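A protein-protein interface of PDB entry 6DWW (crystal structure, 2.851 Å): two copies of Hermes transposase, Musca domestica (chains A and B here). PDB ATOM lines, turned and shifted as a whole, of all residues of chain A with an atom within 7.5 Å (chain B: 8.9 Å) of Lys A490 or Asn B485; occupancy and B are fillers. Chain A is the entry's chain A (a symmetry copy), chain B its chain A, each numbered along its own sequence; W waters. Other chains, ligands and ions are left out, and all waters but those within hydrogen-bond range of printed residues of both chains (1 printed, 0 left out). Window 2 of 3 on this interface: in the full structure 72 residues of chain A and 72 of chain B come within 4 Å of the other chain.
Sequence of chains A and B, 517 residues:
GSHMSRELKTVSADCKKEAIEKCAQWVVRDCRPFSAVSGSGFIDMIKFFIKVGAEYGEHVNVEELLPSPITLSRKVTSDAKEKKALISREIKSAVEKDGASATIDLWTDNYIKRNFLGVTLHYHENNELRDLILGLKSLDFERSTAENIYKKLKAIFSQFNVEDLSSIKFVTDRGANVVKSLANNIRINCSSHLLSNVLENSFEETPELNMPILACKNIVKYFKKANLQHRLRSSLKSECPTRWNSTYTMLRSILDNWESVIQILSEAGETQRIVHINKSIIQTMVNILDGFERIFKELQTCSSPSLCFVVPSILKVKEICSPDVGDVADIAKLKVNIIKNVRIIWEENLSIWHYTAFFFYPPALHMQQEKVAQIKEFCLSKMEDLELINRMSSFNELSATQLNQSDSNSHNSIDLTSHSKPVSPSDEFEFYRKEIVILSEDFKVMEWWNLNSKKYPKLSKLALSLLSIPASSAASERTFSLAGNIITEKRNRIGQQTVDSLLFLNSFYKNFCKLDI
NZ of Lys A490 sits at hydrogen-bond distance from OD1 of Asn B485 (3.5 Å).
OE1 of Glu A489 is in salt-bridge range of NZ of Lys A490 (3.2 Å). The side-chain hydroxyl (OG1) of Thr A488 lies within hydrogen-bond range of the backbone NH (N) of Arg A491.
Among the printed residues, merely in contact across the chains: Cys A31 with Ile B486 and Arg A491 with Pro B33.
Lys A490 touches just one residue of chain B: Asn B485. Of chain A, only Lys A490 comes within 4 Å of Asn B485. No residue of chain A comes within 4 Å of Gly B484. Of the printed residues of chain B, Arg A491 touches Pro B33. Printed residues of chain B within 4 Å of Cys A31: Ile B486. Asn B110 touches none of the printed residues of chain A. Arg B478 touches none of the printed residues of chain A.
Hydrophobic or aromatic side chains of chain B that line the printed part of chain A: Pro B33 and Ile B486. Among the printed residues, no Asp or Glu carboxylate lies within 4 Å of a Lys or Arg side-chain nitrogen of the other chain.
8 positions are printed for both chains.
Water W1 bridges the side-chain amide nitrogen of Asn B485 (3.4 Å) and the side-chain sulfur of Cys A31 (3.7 Å).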
ATOM      1  N   CYS A  31      30.795   2.825   5.759  1.00  0.00           N
ATOM      2  CA  CYS A  31      30.425   2.686   7.167  1.00  0.00           C
ATOM      3  C   CYS A  31      30.231   1.215   7.533  1.00  0.00           C
ATOM      4  O   CYS A  31      29.137   0.759   7.868  1.00  0.00           O
ATOM      5  CB  CYS A  31      29.176   3.510   7.494  1.00  0.00           C
ATOM      6  SG  CYS A  31      28.762   3.573   9.257  1.00  0.00           S
ATOM      7  N   TYR A 111      10.458  -4.775  15.549  1.00  0.00           N
ATOM      8  CA  TYR A 111       9.956  -3.776  14.610  1.00  0.00           C
ATOM      9  C   TYR A 111       8.595  -4.183  14.055  1.00  0.00           C
ATOM     10  O   TYR A 111       7.582  -3.570  14.403  1.00  0.00           O
ATOM     11  CB  TYR A 111      10.966  -3.537  13.482  1.00  0.00           C
ATOM     12  CG  TYR A 111      12.284  -2.967  13.965  1.00  0.00           C
ATOM     13  CD1 TYR A 111      12.476  -1.594  14.068  1.00  0.00           C
ATOM     14  CD2 TYR A 111      13.329  -3.802  14.332  1.00  0.00           C
ATOM     15  CE1 TYR A 111      13.678  -1.069  14.521  1.00  0.00           C
ATOM     16  CE2 TYR A 111      14.531  -3.290  14.787  1.00  0.00           C
ATOM     17  CZ  TYR A 111      14.703  -1.924  14.878  1.00  0.00           C
ATOM     18  OH  TYR A 111      15.902  -1.416  15.328  1.00  0.00           O
ATOM     19  N   ILE A 486      20.070  -9.456  12.377  1.00  0.00           N
ATOM     20  CA  ILE A 486      19.723  -9.224  10.979  1.00  0.00           C
ATOM     21  C   ILE A 486      18.614  -8.192  10.844  1.00  0.00           C
ATOM     22  O   ILE A 486      18.741  -7.225  10.088  1.00  0.00           O
ATOM     23  CB  ILE A 486      19.332 -10.557  10.309  1.00  0.00           C
ATOM     24  CG1 ILE A 486      20.522 -11.517  10.302  1.00  0.00           C
ATOM     25  CG2 ILE A 486      18.824 -10.309   8.903  1.00  0.00           C
ATOM     26  CD1 ILE A 486      20.193 -12.881   9.755  1.00  0.00           C
ATOM     27  N   ILE A 487      17.506  -8.384  11.559  1.00  0.00           N
ATOM     28  CA  ILE A 487      16.390  -7.445  11.518  1.00  0.00           C
ATOM     29  C   ILE A 487      16.744  -6.214  12.341  1.00  0.00           C
ATOM     30  O   ILE A 487      16.384  -6.116  13.518  1.00  0.00           O
ATOM     31  CB  ILE A 487      15.094  -8.092  12.037  1.00  0.00           C
ATOM     32  CG1 ILE A 487      14.969  -9.528  11.526  1.00  0.00           C
ATOM     33  CG2 ILE A 487      13.886  -7.262  11.623  1.00  0.00           C
ATOM     34  CD1 ILE A 487      13.720 -10.236  12.010  1.00  0.00           C
ATOM     35  N   THR A 488      17.445  -5.266  11.733  1.00  0.00           N
ATOM     36  CA  THR A 488      17.964  -4.116  12.447  1.00  0.00           C
ATOM     37  C   THR A 488      17.161  -2.864  12.112  1.00  0.00           C
ATOM     38  O   THR A 488      16.123  -2.914  11.441  1.00  0.00           O
ATOM     39  CB  THR A 488      19.450  -3.918  12.132  1.00  0.00           C
ATOM     40  OG1 THR A 488      19.610  -3.533  10.757  1.00  0.00           O
ATOM     41  CG2 THR A 488      20.216  -5.201  12.404  1.00  0.00           C
ATOM     42  N   GLU A 489      17.656  -1.727  12.598  1.00  0.00           N
ATOM     43  CA  GLU A 489      16.987  -0.453  12.378  1.00  0.00           C
ATOM     44  C   GLU A 489      16.911  -0.119  10.892  1.00  0.00           C
ATOM     45  O   GLU A 489      15.860   0.295  10.390  1.00  0.00           O
ATOM     46  CB  GLU A 489      17.729   0.633  13.150  1.00  0.00           C
ATOM     47  CG  GLU A 489      17.060   1.982  13.209  1.00  0.00           C
ATOM     48  CD  GLU A 489      17.958   3.009  13.866  1.00  0.00           C
ATOM     49  OE1 GLU A 489      18.733   3.674  13.141  1.00  0.00           O
ATOM     50  OE2 GLU A 489      17.910   3.128  15.109  1.00  0.00           O
ATOM     51  N   LYS A 490      18.016  -0.302  10.167  1.00  0.00           N
ATOM     52  CA  LYS A 490      18.051   0.056   8.756  1.00  0.00           C
ATOM     53  C   LYS A 490      17.744  -1.117   7.831  1.00  0.00           C
ATOM     54  O   LYS A 490      17.341  -0.890   6.683  1.00  0.00           O
ATOM     55  CB  LYS A 490      19.414   0.658   8.399  1.00  0.00           C
ATOM     56  CG  LYS A 490      19.959   1.606   9.458  1.00  0.00           C
ATOM     57  CD  LYS A 490      20.535   2.876   8.846  1.00  0.00           C
ATOM     58  CE  LYS A 490      19.481   3.980   8.725  1.00  0.00           C
ATOM     59  NZ  LYS A 490      19.057   4.577  10.036  1.00  0.00           N
ATOM     60  N   ARG A 491      17.918  -2.359   8.291  1.00  0.00           N
ATOM     61  CA  ARG A 491      17.517  -3.537   7.528  1.00  0.00           C
ATOM     62  C   ARG A 491      16.093  -3.979   7.845  1.00  0.00           C
ATOM     63  O   ARG A 491      15.755  -5.155   7.658  1.00  0.00           O
ATOM     64  CB  ARG A 491      18.492  -4.690   7.778  1.00  0.00           C
ATOM     65  CG  ARG A 491      19.935  -4.410   7.371  1.00  0.00           C
ATOM     66  CD  ARG A 491      20.818  -5.634   7.586  1.00  0.00           C
ATOM     67  NE  ARG A 491      20.598  -6.667   6.574  1.00  0.00           N
ATOM     68  CZ  ARG A 491      21.166  -7.869   6.602  1.00  0.00           C
ATOM     69  NH1 ARG A 491      21.980  -8.194   7.593  1.00  0.00           N
ATOM     70  NH2 ARG A 491      20.916  -8.749   5.643  1.00  0.00           N
ATOM     71  N   ASN A 492      15.243  -3.058   8.310  1.00  0.00           N
ATOM     72  CA  ASN A 492      13.941  -3.426   8.858  1.00  0.00           C
ATOM     73  C   ASN A 492      12.976  -3.946   7.800  1.00  0.00           C
ATOM     74  O   ASN A 492      11.999  -4.619   8.153  1.00  0.00           O
ATOM     75  CB  ASN A 492      13.322  -2.224   9.584  1.00  0.00           C
ATOM     76  CG  ASN A 492      12.780  -1.173   8.625  1.00  0.00           C
ATOM     77  OD1 ASN A 492      11.645  -1.274   8.157  1.00  0.00           O
ATOM     78  ND2 ASN A 492      13.579  -0.156   8.341  1.00  0.00           N
ATOM     79  N   ARG A 493      13.214  -3.644   6.522  1.00  0.00           N
ATOM     80  CA  ARG A 493      12.345  -4.107   5.447  1.00  0.00           C
ATOM     81  C   ARG A 493      12.600  -5.557   5.062  1.00  0.00           C
ATOM     82  O   ARG A 493      11.876  -6.087   4.211  1.00  0.00           O
ATOM     83  CB  ARG A 493      12.504  -3.215   4.209  1.00  0.00           C
ATOM     84  CG  ARG A 493      12.072  -1.775   4.418  1.00  0.00           C
ATOM     85  CD  ARG A 493      10.646  -1.697   4.954  1.00  0.00           C
ATOM     86  NE  ARG A 493       9.646  -1.678   3.892  1.00  0.00           N
ATOM     87  CZ  ARG A 493       8.352  -1.905   4.083  1.00  0.00           C
ATOM     88  NH1 ARG A 493       7.899  -2.183   5.300  1.00  0.00           N
ATOM     89  NH2 ARG A 493       7.512  -1.862   3.056  1.00  0.00           N
ATOM     90  N   ILE A 494      13.598  -6.206   5.669  1.00  0.00           N
ATOM     91  CA  ILE A 494      13.964  -7.561   5.281  1.00  0.00           C
ATOM     92  C   ILE A 494      12.793  -8.501   5.532  1.00  0.00           C
ATOM     93  O   ILE A 494      12.039  -8.349   6.503  1.00  0.00           O
ATOM     94  CB  ILE A 494      15.236  -7.995   6.034  1.00  0.00           C
ATOM     95  CG1 ILE A 494      15.976  -9.092   5.275  1.00  0.00           C
ATOM     96  CG2 ILE A 494      14.916  -8.466   7.437  1.00  0.00           C
ATOM     97  CD1 ILE A 494      17.447  -9.162   5.632  1.00  0.00           C
ATOM     98  N   PRO B  33      24.955  -6.661   5.094  1.00  0.00           N
ATOM     99  CA  PRO B  33      23.777  -6.390   4.265  1.00  0.00           C
ATOM    100  C   PRO B  33      24.057  -6.622   2.786  1.00  0.00           C
ATOM    101  O   PRO B  33      25.184  -6.469   2.309  1.00  0.00           O
ATOM    102  CB  PRO B  33      23.477  -4.915   4.549  1.00  0.00           C
ATOM    103  CG  PRO B  33      24.780  -4.349   4.995  1.00  0.00           C
ATOM    104  CD  PRO B  33      25.461  -5.446   5.750  1.00  0.00           C
ATOM    105  N   SER B  35      23.341  -4.792   0.379  1.00  0.00           N
ATOM    106  CA  SER B  35      23.798  -3.561  -0.253  1.00  0.00           C
ATOM    107  C   SER B  35      25.292  -3.312  -0.069  1.00  0.00           C
ATOM    108  O   SER B  35      25.817  -2.358  -0.655  1.00  0.00           O
ATOM    109  CB  SER B  35      23.015  -2.377   0.302  1.00  0.00           C
ATOM    110  OG  SER B  35      23.329  -2.166   1.667  1.00  0.00           O
ATOM    111  N   TRP B 107      24.091  16.942  21.194  1.00  0.00           N
ATOM    112  CA  TRP B 107      23.486  15.627  21.055  1.00  0.00           C
ATOM    113  C   TRP B 107      24.124  14.711  22.082  1.00  0.00           C
ATOM    114  O   TRP B 107      25.266  14.926  22.493  1.00  0.00           O
ATOM    115  CB  TRP B 107      23.684  15.084  19.631  1.00  0.00           C
ATOM    116  CG  TRP B 107      23.307  13.632  19.386  1.00  0.00           C
ATOM    117  CD1 TRP B 107      22.048  13.125  19.224  1.00  0.00           C
ATOM    118  CD2 TRP B 107      24.206  12.520  19.219  1.00  0.00           C
ATOM    119  NE1 TRP B 107      22.106  11.770  18.993  1.00  0.00           N
ATOM    120  CE2 TRP B 107      23.418  11.374  18.984  1.00  0.00           C
ATOM    121  CE3 TRP B 107      25.599  12.381  19.259  1.00  0.00           C
ATOM    122  CZ2 TRP B 107      23.976  10.108  18.791  1.00  0.00           C
ATOM    123  CZ3 TRP B 107      26.153  11.118  19.065  1.00  0.00           C
ATOM    124  CH2 TRP B 107      25.341  10.003  18.835  1.00  0.00           C
ATOM    125  N   ASN B 110      22.974   7.148  22.704  1.00  0.00           N
ATOM    126  CA  ASN B 110      21.958   6.371  23.402  1.00  0.00           C
ATOM    127  C   ASN B 110      22.529   5.312  24.333  1.00  0.00           C
ATOM    128  O   ASN B 110      21.771   4.746  25.126  1.00  0.00           O
ATOM    129  CB  ASN B 110      21.021   5.715  22.384  1.00  0.00           C
ATOM    130  CG  ASN B 110      20.310   6.733  21.506  1.00  0.00           C
ATOM    131  OD1 ASN B 110      20.553   7.936  21.606  1.00  0.00           O
ATOM    132  ND2 ASN B 110      19.433   6.251  20.633  1.00  0.00           N
ATOM    133  N   TYR B 111      23.832   5.036  24.273  1.00  0.00           N
ATOM    134  CA  TYR B 111      24.443   3.994  25.092  1.00  0.00           C
ATOM    135  C   TYR B 111      25.296   4.601  26.201  1.00  0.00           C
ATOM    136  O   TYR B 111      24.915   4.536  27.373  1.00  0.00           O
ATOM    137  CB  TYR B 111      25.265   3.035  24.223  1.00  0.00           C
ATOM    138  CG  TYR B 111      24.430   2.273  23.213  1.00  0.00           C
ATOM    139  CD1 TYR B 111      23.845   1.055  23.539  1.00  0.00           C
ATOM    140  CD2 TYR B 111      24.216   2.782  21.940  1.00  0.00           C
ATOM    141  CE1 TYR B 111      23.071   0.362  22.619  1.00  0.00           C
ATOM    142  CE2 TYR B 111      23.445   2.100  21.015  1.00  0.00           C
ATOM    143  CZ  TYR B 111      22.876   0.891  21.357  1.00  0.00           C
ATOM    144  OH  TYR B 111      22.110   0.212  20.434  1.00  0.00           O
ATOM    145  N   ARG B 478      21.776  15.856  10.956  1.00  0.00           N
ATOM    146  CA  ARG B 478      22.164  14.702  10.148  1.00  0.00           C
ATOM    147  C   ARG B 478      23.472  14.098  10.631  1.00  0.00           C
ATOM    148  O   ARG B 478      23.656  12.877  10.573  1.00  0.00           O
ATOM    149  CB  ARG B 478      22.282  15.103   8.682  1.00  0.00           C
ATOM    150  CG  ARG B 478      20.971  15.117   7.957  1.00  0.00           C
ATOM    151  CD  ARG B 478      21.148  15.580   6.533  1.00  0.00           C
ATOM    152  NE  ARG B 478      20.479  16.854   6.308  1.00  0.00           N
ATOM    153  CZ  ARG B 478      21.099  17.964   5.928  1.00  0.00           C
ATOM    154  NH1 ARG B 478      22.407  17.954   5.710  1.00  0.00           N
ATOM    155  NH2 ARG B 478      20.404  19.080   5.753  1.00  0.00           N
ATOM    156  N   THR B 479      24.397  14.940  11.100  1.00  0.00           N
ATOM    157  CA  THR B 479      25.642  14.431  11.667  1.00  0.00           C
ATOM    158  C   THR B 479      25.360  13.489  12.829  1.00  0.00           C
ATOM    159  O   THR B 479      26.023  12.454  12.977  1.00  0.00           O
ATOM    160  CB  THR B 479      26.527  15.592  12.129  1.00  0.00           C
ATOM    161  OG1 THR B 479      26.725  16.513  11.050  1.00  0.00           O
ATOM    162  CG2 THR B 479      27.875  15.078  12.598  1.00  0.00           C
ATOM    163  N   PHE B 480      24.368  13.830  13.658  1.00  0.00           N
ATOM    164  CA  PHE B 480      23.988  12.972  14.774  1.00  0.00           C
ATOM    165  C   PHE B 480      23.341  11.684  14.282  1.00  0.00           C
ATOM    166  O   PHE B 480      23.521  10.620  14.886  1.00  0.00           O
ATOM    167  CB  PHE B 480      23.049  13.730  15.710  1.00  0.00           C
ATOM    168  CG  PHE B 480      23.602  15.045  16.189  1.00  0.00           C
ATOM    169  CD1 PHE B 480      22.767  16.131  16.390  1.00  0.00           C
ATOM    170  CD2 PHE B 480      24.957  15.195  16.440  1.00  0.00           C
ATOM    171  CE1 PHE B 480      23.271  17.341  16.828  1.00  0.00           C
ATOM    172  CE2 PHE B 480      25.465  16.403  16.882  1.00  0.00           C
ATOM    173  CZ  PHE B 480      24.620  17.478  17.076  1.00  0.00           C
ATOM    174  N   SER B 481      22.588  11.756  13.183  1.00  0.00           N
ATOM    175  CA  SER B 481      22.040  10.543  12.589  1.00  0.00           C
ATOM    176  C   SER B 481      23.159   9.641  12.094  1.00  0.00           C
ATOM    177  O   SER B 481      23.157   8.430  12.349  1.00  0.00           O
ATOM    178  CB  SER B 481      21.084  10.898  11.453  1.00  0.00           C
ATOM    179  OG  SER B 481      20.356   9.760  11.024  1.00  0.00           O
ATOM    180  N   LEU B 482      24.137  10.222  11.391  1.00  0.00           N
ATOM    181  CA  LEU B 482      25.301   9.452  10.966  1.00  0.00           C
ATOM    182  C   LEU B 482      26.065   8.905  12.163  1.00  0.00           C
ATOM    183  O   LEU B 482      26.459   7.732  12.174  1.00  0.00           O
ATOM    184  CB  LEU B 482      26.214  10.314  10.096  1.00  0.00           C
ATOM    185  CG  LEU B 482      25.701  10.668   8.698  1.00  0.00           C
ATOM    186  CD1 LEU B 482      26.643  11.644   8.034  1.00  0.00           C
ATOM    187  CD2 LEU B 482      25.527   9.420   7.843  1.00  0.00           C
ATOM    188  N   ALA B 483      26.274   9.737  13.184  1.00  0.00           N
ATOM    189  CA  ALA B 483      26.929   9.274  14.402  1.00  0.00           C
ATOM    190  C   ALA B 483      26.227   8.048  14.964  1.00  0.00           C
ATOM    191  O   ALA B 483      26.867   7.049  15.309  1.00  0.00           O
ATOM    192  CB  ALA B 483      26.952  10.400  15.436  1.00  0.00           C
ATOM    193  N   GLY B 484      24.897   8.105  15.047  1.00  0.00           N
ATOM    194  CA  GLY B 484      24.120   6.984  15.539  1.00  0.00           C
ATOM    195  C   GLY B 484      24.194   5.742  14.675  1.00  0.00           C
ATOM    196  O   GLY B 484      23.976   4.636  15.182  1.00  0.00           O
ATOM    197  N   ASN B 485      24.479   5.898  13.379  1.00  0.00           N
ATOM    198  CA  ASN B 485      24.715   4.725  12.543  1.00  0.00           C
ATOM    199  C   ASN B 485      26.029   4.026  12.885  1.00  0.00           C
ATOM    200  O   ASN B 485      26.207   2.855  12.528  1.00  0.00           O
ATOM    201  CB  ASN B 485      24.712   5.097  11.061  1.00  0.00           C
ATOM    202  CG  ASN B 485      23.331   5.439  10.541  1.00  0.00           C
ATOM    203  OD1 ASN B 485      22.323   4.997  11.082  1.00  0.00           O
ATOM    204  ND2 ASN B 485      23.283   6.229   9.470  1.00  0.00           N
ATOM    205  N   ILE B 486      26.944   4.708  13.569  1.00  0.00           N
ATOM    206  CA  ILE B 486      28.219   4.112  13.956  1.00  0.00           C
ATOM    207  C   ILE B 486      28.160   3.539  15.364  1.00  0.00           C
ATOM    208  O   ILE B 486      28.521   2.381  15.589  1.00  0.00           O
ATOM    209  CB  ILE B 486      29.347   5.154  13.822  1.00  0.00           C
ATOM    210  CG1 ILE B 486      29.502   5.585  12.363  1.00  0.00           C
ATOM    211  CG2 ILE B 486      30.646   4.595  14.365  1.00  0.00           C
ATOM    212  CD1 ILE B 486      30.517   6.679  12.162  1.00  0.00           C
ATOM    213  N   ILE B 487      27.722   4.339  16.336  1.00  0.00           N
ATOM    214  CA  ILE B 487      27.608   3.885  17.717  1.00  0.00           C
ATOM    215  C   ILE B 487      26.377   2.999  17.850  1.00  0.00           C
ATOM    216  O   ILE B 487      25.302   3.466  18.238  1.00  0.00           O
ATOM    217  CB  ILE B 487      27.534   5.071  18.693  1.00  0.00           C
ATOM    218  CG1 ILE B 487      28.509   6.172  18.276  1.00  0.00           C
ATOM    219  CG2 ILE B 487      27.817   4.605  20.115  1.00  0.00           C
ATOM    220  CD1 ILE B 487      28.480   7.383  19.186  1.00  0.00           C
ATOM    221  N   THR B 488      26.522   1.718  17.537  1.00  0.00           N
ATOM    222  CA  THR B 488      25.395   0.807  17.485  1.00  0.00           C
ATOM    223  C   THR B 488      25.404  -0.132  18.686  1.00  0.00           C
ATOM    224  O   THR B 488      26.197   0.014  19.623  1.00  0.00           O
ATOM    225  CB  THR B 488      25.404   0.021  16.170  1.00  0.00           C
ATOM    226  OG1 THR B 488      26.530  -0.871  16.142  1.00  0.00           O
ATOM    227  CG2 THR B 488      25.469   0.976  14.992  1.00  0.00           C
ATOM    228  N   GLU B 489      24.498  -1.107  18.649  1.00  0.00           N
ATOM    229  CA  GLU B 489      24.373  -2.069  19.735  1.00  0.00           C
ATOM    230  C   GLU B 489      25.654  -2.877  19.906  1.00  0.00           C
ATOM    231  O   GLU B 489      26.137  -3.067  21.028  1.00  0.00           O
ATOM    232  CB  GLU B 489      23.180  -2.978  19.453  1.00  0.00           C
ATOM    233  CG  GLU B 489      22.770  -3.902  20.570  1.00  0.00           C
ATOM    234  CD  GLU B 489      21.683  -4.854  20.120  1.00  0.00           C
ATOM    235  OE1 GLU B 489      22.020  -5.957  19.633  1.00  0.00           O
ATOM    236  OE2 GLU B 489      20.493  -4.486  20.227  1.00  0.00           O
ATOM    237  N   LYS B 490      26.228  -3.355  18.800  1.00  0.00           N
ATOM    238  CA  LYS B 490      27.416  -4.195  18.879  1.00  0.00           C
ATOM    239  C   LYS B 490      28.715  -3.412  18.721  1.00  0.00           C
ATOM    240  O   LYS B 490      29.766  -3.894  19.162  1.00  0.00           O
ATOM    241  CB  LYS B 490      27.346  -5.305  17.825  1.00  0.00           C
ATOM    242  CG  LYS B 490      25.962  -5.923  17.680  1.00  0.00           C
ATOM    243  CD  LYS B 490      26.020  -7.443  17.601  1.00  0.00           C
ATOM    244  CE  LYS B 490      25.917  -8.091  18.985  1.00  0.00           C
ATOM    245  NZ  LYS B 490      24.558  -7.987  19.617  1.00  0.00           N
ATOM    246  N   ARG B 491      28.678  -2.224  18.111  1.00  0.00           N
ATOM    247  CA  ARG B 491      29.843  -1.347  18.041  1.00  0.00           C
ATOM    248  C   ARG B 491      29.905  -0.368  19.209  1.00  0.00           C
ATOM    249  O   ARG B 491      30.524   0.697  19.090  1.00  0.00           O
ATOM    250  CB  ARG B 491      29.854  -0.583  16.715  1.00  0.00           C
ATOM    251  CG  ARG B 491      29.927  -1.459  15.470  1.00  0.00           C
ATOM    252  CD  ARG B 491      30.009  -0.614  14.203  1.00  0.00           C
ATOM    253  NE  ARG B 491      31.329  -0.015  14.015  1.00  0.00           N
ATOM    254  CZ  ARG B 491      31.624   0.848  13.047  1.00  0.00           C
ATOM    255  NH1 ARG B 491      30.692   1.220  12.184  1.00  0.00           N
ATOM    256  NH2 ARG B 491      32.849   1.345  12.943  1.00  0.00           N
ATOM    257  N   ILE B 494      33.044   1.605  20.683  1.00  0.00           N
ATOM    258  CA  ILE B 494      33.806   2.515  19.841  1.00  0.00           C
ATOM    259  C   ILE B 494      34.060   3.816  20.590  1.00  0.00           C
ATOM    260  O   ILE B 494      33.217   4.294  21.361  1.00  0.00           O
ATOM    261  CB  ILE B 494      33.065   2.740  18.510  1.00  0.00           C
ATOM    262  CG1 ILE B 494      34.031   3.167  17.408  1.00  0.00           C
ATOM    263  CG2 ILE B 494      31.965   3.771  18.655  1.00  0.00           C
ATOM    264  CD1 ILE B 494      33.506   2.864  16.019  1.00  0.00           C
ATOM    265  N   VAL B 499      34.843   7.871  16.363  1.00  0.00           N
ATOM    266  CA  VAL B 499      33.655   8.351  15.666  1.00  0.00           C
ATOM    267  C   VAL B 499      33.940   9.683  14.991  1.00  0.00           C
ATOM    268  O   VAL B 499      33.531   9.909  13.846  1.00  0.00           O
ATOM    269  CB  VAL B 499      32.468   8.459  16.640  1.00  0.00           C
ATOM    270  CG1 VAL B 499      31.213   8.911  15.902  1.00  0.00           C
ATOM    271  CG2 VAL B 499      32.235   7.133  17.347  1.00  0.00           C
ATOM    272  N   LEU B 502      35.904   8.750  11.769  1.00  0.00           N
ATOM    273  CA  LEU B 502      35.133   8.096  10.717  1.00  0.00           C
ATOM    274  C   LEU B 502      34.145   9.054  10.070  1.00  0.00           C
ATOM    275  O   LEU B 502      33.957   9.029   8.848  1.00  0.00           O
ATOM    276  CB  LEU B 502      34.397   6.889  11.286  1.00  0.00           C
ATOM    277  CG  LEU B 502      35.234   5.634  11.492  1.00  0.00           C
ATOM    278  CD1 LEU B 502      34.560   4.735  12.514  1.00  0.00           C
ATOM    279  CD2 LEU B 502      35.415   4.913  10.161  1.00  0.00           C
ATOM    280  N   LEU B 503      33.495   9.897  10.874  1.00  0.00           N
ATOM    281  CA  LEU B 503      32.519  10.837  10.331  1.00  0.00           C
ATOM    282  C   LEU B 503      33.181  11.845   9.402  1.00  0.00           C
ATOM    283  O   LEU B 503      32.681  12.115   8.304  1.00  0.00           O
ATOM    284  CB  LEU B 503      31.792  11.555  11.469  1.00  0.00           C
ATOM    285  CG  LEU B 503      30.733  10.766  12.235  1.00  0.00           C
ATOM    286  CD1 LEU B 503      30.082  11.651  13.280  1.00  0.00           C
ATOM    287  CD2 LEU B 503      29.696  10.219  11.277  1.00  0.00           C
HETATM  288  O   HOH W   1      26.363   6.154   8.015  1.00  0.00           O
